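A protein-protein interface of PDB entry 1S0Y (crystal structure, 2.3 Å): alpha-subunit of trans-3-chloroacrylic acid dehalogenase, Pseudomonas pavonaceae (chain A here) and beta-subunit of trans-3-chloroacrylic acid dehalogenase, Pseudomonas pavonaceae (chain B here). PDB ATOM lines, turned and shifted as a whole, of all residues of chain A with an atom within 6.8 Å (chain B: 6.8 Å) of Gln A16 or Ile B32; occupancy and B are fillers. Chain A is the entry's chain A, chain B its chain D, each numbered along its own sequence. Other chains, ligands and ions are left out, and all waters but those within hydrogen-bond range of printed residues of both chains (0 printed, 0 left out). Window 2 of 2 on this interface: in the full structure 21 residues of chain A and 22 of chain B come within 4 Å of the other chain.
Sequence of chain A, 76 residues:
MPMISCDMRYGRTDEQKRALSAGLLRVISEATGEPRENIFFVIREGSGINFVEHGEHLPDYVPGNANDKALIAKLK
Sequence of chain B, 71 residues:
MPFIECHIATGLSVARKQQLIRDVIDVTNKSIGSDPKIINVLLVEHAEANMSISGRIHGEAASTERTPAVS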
ATOM      1  N   CYS A   6      13.853  17.188 -14.973  1.00  0.00           N
ATOM      2  CA  CYS A   6      13.415  16.684 -16.259  1.00  0.00           C
ATOM      3  C   CYS A   6      12.915  15.254 -16.132  1.00  0.00           C
ATOM      4  O   CYS A   6      13.701  14.325 -15.981  1.00  0.00           O
ATOM      5  CB  CYS A   6      14.548  16.730 -17.277  1.00  0.00           C
ATOM      6  SG  CYS A   6      14.113  15.859 -18.799  1.00  0.00           S
ATOM      7  N   MET A   8      11.719  12.150 -17.730  1.00  0.00           N
ATOM      8  CA  MET A   8      11.663  11.509 -19.039  1.00  0.00           C
ATOM      9  C   MET A   8      11.767   9.996 -18.952  1.00  0.00           C
ATOM     10  O   MET A   8      12.200   9.464 -17.939  1.00  0.00           O
ATOM     11  CB  MET A   8      12.751  12.069 -19.964  1.00  0.00           C
ATOM     12  CG  MET A   8      14.163  11.661 -19.644  1.00  0.00           C
ATOM     13  SD  MET A   8      15.284  12.522 -20.759  1.00  0.00           S
ATOM     14  CE  MET A   8      16.921  12.082 -20.016  1.00  0.00           C
ATOM     15  N   GLY A  11      16.120   4.854 -20.616  1.00  0.00           N
ATOM     16  CA  GLY A  11      16.751   4.561 -21.892  1.00  0.00           C
ATOM     17  C   GLY A  11      17.811   5.520 -22.400  1.00  0.00           C
ATOM     18  O   GLY A  11      18.732   5.105 -23.106  1.00  0.00           O
ATOM     19  N   ARG A  12      17.681   6.798 -22.061  1.00  0.00           N
ATOM     20  CA  ARG A  12      18.646   7.789 -22.502  1.00  0.00           C
ATOM     21  C   ARG A  12      20.052   7.459 -21.969  1.00  0.00           C
ATOM     22  O   ARG A  12      20.219   7.111 -20.795  1.00  0.00           O
ATOM     23  CB  ARG A  12      18.203   9.178 -22.028  1.00  0.00           C
ATOM     24  CG  ARG A  12      17.834  10.150 -23.139  1.00  0.00           C
ATOM     25  CD  ARG A  12      16.591   9.747 -23.936  1.00  0.00           C
ATOM     26  NE  ARG A  12      15.401   9.572 -23.112  1.00  0.00           N
ATOM     27  CZ  ARG A  12      14.162   9.849 -23.516  1.00  0.00           C
ATOM     28  NH1 ARG A  12      13.136   9.648 -22.698  1.00  0.00           N
ATOM     29  NH2 ARG A  12      13.942  10.347 -24.727  1.00  0.00           N
ATOM     30  N   THR A  13      21.059   7.574 -22.833  1.00  0.00           N
ATOM     31  CA  THR A  13      22.438   7.271 -22.445  1.00  0.00           C
ATOM     32  C   THR A  13      23.077   8.352 -21.580  1.00  0.00           C
ATOM     33  O   THR A  13      22.575   9.467 -21.503  1.00  0.00           O
ATOM     34  CB  THR A  13      23.348   7.091 -23.676  1.00  0.00           C
ATOM     35  OG1 THR A  13      23.680   8.381 -24.218  1.00  0.00           O
ATOM     36  CG2 THR A  13      22.643   6.265 -24.740  1.00  0.00           C
ATOM     37  N   ASP A  14      24.186   8.006 -20.933  1.00  0.00           N
ATOM     38  CA  ASP A  14      24.929   8.949 -20.103  1.00  0.00           C
ATOM     39  C   ASP A  14      25.345  10.132 -20.981  1.00  0.00           C
ATOM     40  O   ASP A  14      25.304  11.287 -20.555  1.00  0.00           O
ATOM     41  CB  ASP A  14      26.198   8.298 -19.541  1.00  0.00           C
ATOM     42  CG  ASP A  14      25.925   7.326 -18.405  1.00  0.00           C
ATOM     43  OD1 ASP A  14      26.884   6.631 -18.008  1.00  0.00           O
ATOM     44  OD2 ASP A  14      24.777   7.256 -17.904  1.00  0.00           O
ATOM     45  N   GLU A  15      25.757   9.832 -22.208  1.00  0.00           N
ATOM     46  CA  GLU A  15      26.178  10.867 -23.145  1.00  0.00           C
ATOM     47  C   GLU A  15      25.038  11.864 -23.372  1.00  0.00           C
ATOM     48  O   GLU A  15      25.220  13.070 -23.238  1.00  0.00           O
ATOM     49  CB  GLU A  15      26.609  10.228 -24.462  1.00  0.00           C
ATOM     50  N   GLN A  16      23.859  11.356 -23.699  1.00  0.00           N
ATOM     51  CA  GLN A  16      22.700  12.212 -23.927  1.00  0.00           C
ATOM     52  C   GLN A  16      22.342  13.060 -22.701  1.00  0.00           C
ATOM     53  O   GLN A  16      21.873  14.184 -22.837  1.00  0.00           O
ATOM     54  CB  GLN A  16      21.485  11.362 -24.312  1.00  0.00           C
ATOM     55  CG  GLN A  16      21.585  10.682 -25.660  1.00  0.00           C
ATOM     56  CD  GLN A  16      20.514   9.625 -25.848  1.00  0.00           C
ATOM     57  OE1 GLN A  16      20.619   8.527 -25.315  1.00  0.00           O
ATOM     58  NE2 GLN A  16      19.470   9.959 -26.593  1.00  0.00           N
ATOM     59  N   LYS A  17      22.566  12.525 -21.505  1.00  0.00           N
ATOM     60  CA  LYS A  17      22.226  13.253 -20.282  1.00  0.00           C
ATOM     61  C   LYS A  17      23.159  14.413 -19.932  1.00  0.00           C
ATOM     62  O   LYS A  17      22.720  15.412 -19.357  1.00  0.00           O
ATOM     63  CB  LYS A  17      22.147  12.282 -19.098  1.00  0.00           C
ATOM     64  CG  LYS A  17      20.996  11.291 -19.173  1.00  0.00           C
ATOM     65  CD  LYS A  17      21.043  10.317 -18.000  1.00  0.00           C
ATOM     66  CE  LYS A  17      19.849   9.382 -17.976  1.00  0.00           C
ATOM     67  NZ  LYS A  17      19.999   8.393 -16.859  1.00  0.00           N
ATOM     68  N   ARG A  18      24.441  14.290 -20.252  1.00  0.00           N
ATOM     69  CA  ARG A  18      25.371  15.375 -19.959  1.00  0.00           C
ATOM     70  C   ARG A  18      25.245  16.458 -21.028  1.00  0.00           C
ATOM     71  O   ARG A  18      25.554  17.624 -20.789  1.00  0.00           O
ATOM     72  CB  ARG A  18      26.805  14.846 -19.879  1.00  0.00           C
ATOM     73  CG  ARG A  18      27.027  13.552 -20.631  1.00  0.00           C
ATOM     74  CD  ARG A  18      28.376  12.963 -20.278  1.00  0.00           C
ATOM     75  NE  ARG A  18      28.656  13.173 -18.866  1.00  0.00           N
ATOM     76  CZ  ARG A  18      29.441  12.394 -18.136  1.00  0.00           C
ATOM     77  NH1 ARG A  18      30.025  11.342 -18.695  1.00  0.00           N
ATOM     78  NH2 ARG A  18      29.642  12.669 -16.849  1.00  0.00           N
ATOM     79  N   ALA A  19      24.775  16.057 -22.205  1.00  0.00           N
ATOM     80  CA  ALA A  19      24.561  16.992 -23.297  1.00  0.00           C
ATOM     81  C   ALA A  19      23.308  17.772 -22.897  1.00  0.00           C
ATOM     82  O   ALA A  19      23.231  18.993 -23.051  1.00  0.00           O
ATOM     83  CB  ALA A  19      24.331  16.234 -24.609  1.00  0.00           C
ATOM     84  N   LEU A  20      22.325  17.050 -22.369  1.00  0.00           N
ATOM     85  CA  LEU A  20      21.086  17.669 -21.925  1.00  0.00           C
ATOM     86  C   LEU A  20      21.381  18.686 -20.825  1.00  0.00           C
ATOM     87  O   LEU A  20      20.969  19.845 -20.911  1.00  0.00           O
ATOM     88  CB  LEU A  20      20.124  16.609 -21.397  1.00  0.00           C
ATOM     89  CG  LEU A  20      18.783  17.143 -20.894  1.00  0.00           C
ATOM     90  CD1 LEU A  20      18.051  17.815 -22.040  1.00  0.00           C
ATOM     91  CD2 LEU A  20      17.959  16.003 -20.330  1.00  0.00           C
ATOM     92  N   SER A  21      22.110  18.251 -19.799  1.00  0.00           N
ATOM     93  CA  SER A  21      22.449  19.126 -18.681  1.00  0.00           C
ATOM     94  C   SER A  21      23.312  20.304 -19.120  1.00  0.00           C
ATOM     95  O   SER A  21      23.095  21.438 -18.692  1.00  0.00           O
ATOM     96  CB  SER A  21      23.169  18.336 -17.589  1.00  0.00           C
ATOM     97  OG  SER A  21      24.307  17.684 -18.114  1.00  0.00           O
ATOM     98  N   TYR A  61      11.001   3.792 -24.198  1.00  0.00           N
ATOM     99  CA  TYR A  61      12.001   4.468 -25.010  1.00  0.00           C
ATOM    100  C   TYR A  61      13.012   3.462 -25.539  1.00  0.00           C
ATOM    101  O   TYR A  61      13.431   2.552 -24.819  1.00  0.00           O
ATOM    102  CB  TYR A  61      12.734   5.528 -24.188  1.00  0.00           C
ATOM    103  CG  TYR A  61      13.847   6.211 -24.951  1.00  0.00           C
ATOM    104  CD1 TYR A  61      13.567   7.091 -25.998  1.00  0.00           C
ATOM    105  CD2 TYR A  61      15.181   5.952 -24.651  1.00  0.00           C
ATOM    106  CE1 TYR A  61      14.593   7.696 -26.729  1.00  0.00           C
ATOM    107  CE2 TYR A  61      16.211   6.546 -25.374  1.00  0.00           C
ATOM    108  CZ  TYR A  61      15.911   7.416 -26.408  1.00  0.00           C
ATOM    109  OH  TYR A  61      16.934   8.000 -27.110  1.00  0.00           O
ATOM    110  N   PRO A  63      16.754   3.261 -27.215  1.00  0.00           N
ATOM    111  CA  PRO A  63      17.985   3.966 -27.583  1.00  0.00           C
ATOM    112  C   PRO A  63      18.624   3.379 -28.840  1.00  0.00           C
ATOM    113  O   PRO A  63      19.803   2.983 -28.768  1.00  0.00           O
ATOM    114  CB  PRO A  63      18.858   3.789 -26.346  1.00  0.00           C
ATOM    115  CG  PRO A  63      18.477   2.419 -25.880  1.00  0.00           C
ATOM    116  CD  PRO A  63      16.966   2.412 -26.027  1.00  0.00           C
ATOM    117  N   PRO B   2      10.279  14.243 -22.502  1.00  0.00           N
ATOM    118  CA  PRO B   2      10.723  15.171 -21.456  1.00  0.00           C
ATOM    119  C   PRO B   2       9.728  16.215 -20.973  1.00  0.00           C
ATOM    120  O   PRO B   2       9.095  16.919 -21.769  1.00  0.00           O
ATOM    121  CB  PRO B   2      11.999  15.785 -22.028  1.00  0.00           C
ATOM    122  CG  PRO B   2      11.860  15.623 -23.480  1.00  0.00           C
ATOM    123  CD  PRO B   2      11.153  14.329 -23.686  1.00  0.00           C
ATOM    124  N   VAL B  27      17.107  23.294 -26.861  1.00  0.00           N
ATOM    125  CA  VAL B  27      18.303  22.643 -26.341  1.00  0.00           C
ATOM    126  C   VAL B  27      18.059  21.178 -26.006  1.00  0.00           C
ATOM    127  O   VAL B  27      18.982  20.362 -26.034  1.00  0.00           O
ATOM    128  CB  VAL B  27      18.837  23.380 -25.097  1.00  0.00           C
ATOM    129  CG1 VAL B  27      18.003  23.031 -23.878  1.00  0.00           C
ATOM    130  CG2 VAL B  27      20.295  23.036 -24.885  1.00  0.00           C
ATOM    131  N   THR B  28      16.812  20.848 -25.695  1.00  0.00           N
ATOM    132  CA  THR B  28      16.448  19.476 -25.379  1.00  0.00           C
ATOM    133  C   THR B  28      16.400  18.697 -26.680  1.00  0.00           C
ATOM    134  O   THR B  28      17.074  17.677 -26.838  1.00  0.00           O
ATOM    135  CB  THR B  28      15.062  19.405 -24.722  1.00  0.00           C
ATOM    136  OG1 THR B  28      15.115  20.023 -23.434  1.00  0.00           O
ATOM    137  CG2 THR B  28      14.610  17.963 -24.580  1.00  0.00           C
ATOM    138  N   ASN B  29      15.598  19.197 -27.613  1.00  0.00           N
ATOM    139  CA  ASN B  29      15.445  18.559 -28.914  1.00  0.00           C
ATOM    140  C   ASN B  29      16.782  18.275 -29.575  1.00  0.00           C
ATOM    141  O   ASN B  29      16.976  17.213 -30.162  1.00  0.00           O
ATOM    142  CB  ASN B  29      14.598  19.436 -29.840  1.00  0.00           C
ATOM    143  CG  ASN B  29      14.803  19.099 -31.310  1.00  0.00           C
ATOM    144  OD1 ASN B  29      15.804  19.487 -31.916  1.00  0.00           O
ATOM    145  ND2 ASN B  29      13.858  18.365 -31.884  1.00  0.00           N
ATOM    146  N   LYS B  30      17.704  19.222 -29.470  1.00  0.00           N
ATOM    147  CA  LYS B  30      19.010  19.063 -30.083  1.00  0.00           C
ATOM    148  C   LYS B  30      19.909  18.064 -29.362  1.00  0.00           C
ATOM    149  O   LYS B  30      20.645  17.316 -30.005  1.00  0.00           O
ATOM    150  CB  LYS B  30      19.705  20.422 -30.180  1.00  0.00           C
ATOM    151  N   SER B  31      19.842  18.038 -28.033  1.00  0.00           N
ATOM    152  CA  SER B  31      20.694  17.139 -27.253  1.00  0.00           C
ATOM    153  C   SER B  31      20.119  15.756 -26.960  1.00  0.00           C
ATOM    154  O   SER B  31      20.859  14.842 -26.597  1.00  0.00           O
ATOM    155  CB  SER B  31      21.090  17.805 -25.929  1.00  0.00           C
ATOM    156  OG  SER B  31      19.961  18.069 -25.115  1.00  0.00           O
ATOM    157  N   ILE B  32      18.811  15.597 -27.117  1.00  0.00           N
ATOM    158  CA  ILE B  32      18.173  14.314 -26.839  1.00  0.00           C
ATOM    159  C   ILE B  32      17.444  13.758 -28.059  1.00  0.00           C
ATOM    160  O   ILE B  32      17.098  12.576 -28.104  1.00  0.00           O
ATOM    161  CB  ILE B  32      17.201  14.449 -25.628  1.00  0.00           C
ATOM    162  CG1 ILE B  32      17.987  14.292 -24.327  1.00  0.00           C
ATOM    163  CG2 ILE B  32      16.088  13.433 -25.697  1.00  0.00           C
ATOM    164  CD1 ILE B  32      17.112  14.318 -23.082  1.00  0.00           C
ATOM    165  N   GLY B  33      17.225  14.615 -29.051  1.00  0.00           N
ATOM    166  CA  GLY B  33      16.552  14.185 -30.263  1.00  0.00           C
ATOM    167  C   GLY B  33      15.064  13.949 -30.095  1.00  0.00           C
ATOM    168  O   GLY B  33      14.461  13.190 -30.855  1.00  0.00           O
ATOM    169  N   SER B  34      14.467  14.597 -29.103  1.00  0.00           N
ATOM    170  CA  SER B  34      13.040  14.447 -28.848  1.00  0.00           C
ATOM    171  C   SER B  34      12.231  15.440 -29.666  1.00  0.00           C
ATOM    172  O   SER B  34      12.567  16.617 -29.726  1.00  0.00           O
ATOM    173  CB  SER B  34      12.737  14.665 -27.358  1.00  0.00           C
ATOM    174  OG  SER B  34      13.235  13.604 -26.562  1.00  0.00           O
ATOM    175  N   ASP B  35      11.160  14.959 -30.287  1.00  0.00           N
ATOM    176  CA  ASP B  35      10.285  15.814 -31.078  1.00  0.00           C
ATOM    177  C   ASP B  35       9.606  16.795 -30.123  1.00  0.00           C
ATOM    178  O   ASP B  35       9.017  16.382 -29.127  1.00  0.00           O
ATOM    179  CB  ASP B  35       9.215  14.973 -31.774  1.00  0.00           C
ATOM    180  CG  ASP B  35       8.324  15.799 -32.681  1.00  0.00           C
ATOM    181  OD1 ASP B  35       7.830  16.857 -32.238  1.00  0.00           O
ATOM    182  OD2 ASP B  35       8.111  15.389 -33.841  1.00  0.00           O
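Printed residues of chain B that touch a printed residue of chain A: Pro B2, Thr B28, Ser B31, Ile B32 and Ser B34. Of the 15 printed residues of chain A, 6 touch a printed residue of chain B. Hydrophobic or aromatic side chains of chain A that line the printed part of chain B: Met A8, Ala A19 and Leu A20. Along chain A the printed residues that touch a printed residue of chain B span positions 6 to 20. Among the printed residues, 11 pairs touch across the chains. Among the printed residues, no Asp or Glu carboxylate lies within 4 Å of a Lys or Arg side-chain nitrogen of the other chain.
NE of Arg A12 lies within hydrogen-bond range of SD of Met A8 (3.8 Å). The side-chain amide oxygen (OE1) of Gln A16 sits at hydrogen-bond distance from the backbone NH (N) of Thr A13 (2.7 Å). OH of Tyr A61 sits at hydrogen-bond distance from NE2 of Gln A16 (3.2 Å). O of Val B27 is in hydrogen-bond range of OG of Ser B31 (2.7 Å). The backbone carbonyl oxygen (O) of Thr B28 lies within hydrogen-bond range of the side-chain hydroxyl (OG) of Ser B31 (3.4 Å). ND2 of Asn B29 lies within hydrogen-bond range of O of Ser B34 (3.1 Å).
Cys A6 touches Pro B2 (SG to CB, 3.9 Å). Met A8 touches Pro B2 (CB to CA, 3.995 Å). CD1 of Ile B32 touches SD of Met A8, 3.5 Å away. NH2 of Arg A12 touches CG2 of Ile B32 (3.9 Å). Ser B34 touches Arg A12 (OG to NH2, 3.8 Å). Gln A16 touches Ser B31. C of Ala A19 touches CB of Ser B31 (3.8 Å). Thr B28 touches Leu A20. CA of Leu A20 touches OG of Ser B31, at 3.4 Å. Leu A20 touches Ile B32 (CD2 to CD1, 3.3 Å).
Of the printed residues of chain B, Met A8 touches Pro B2 and Ile B32. Printed residues of chain B within 4 Å of Ala A19: Ser B31 (3.8 Å). Pro A63 touches none of the printed residues of chain B. Printed residues of chain A within 4 Å of Pro B2: Cys A6 and Met A8. Ile B32 touches just these residues of chain A: Met A8 (3.5 Å), Arg A12 (3.9 Å), Gln A16 (3.8 Å) and Leu A20 (3.3 Å). The nearest residue of chain A that does not touch Ile B32 is Tyr A61 (4.7 Å).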
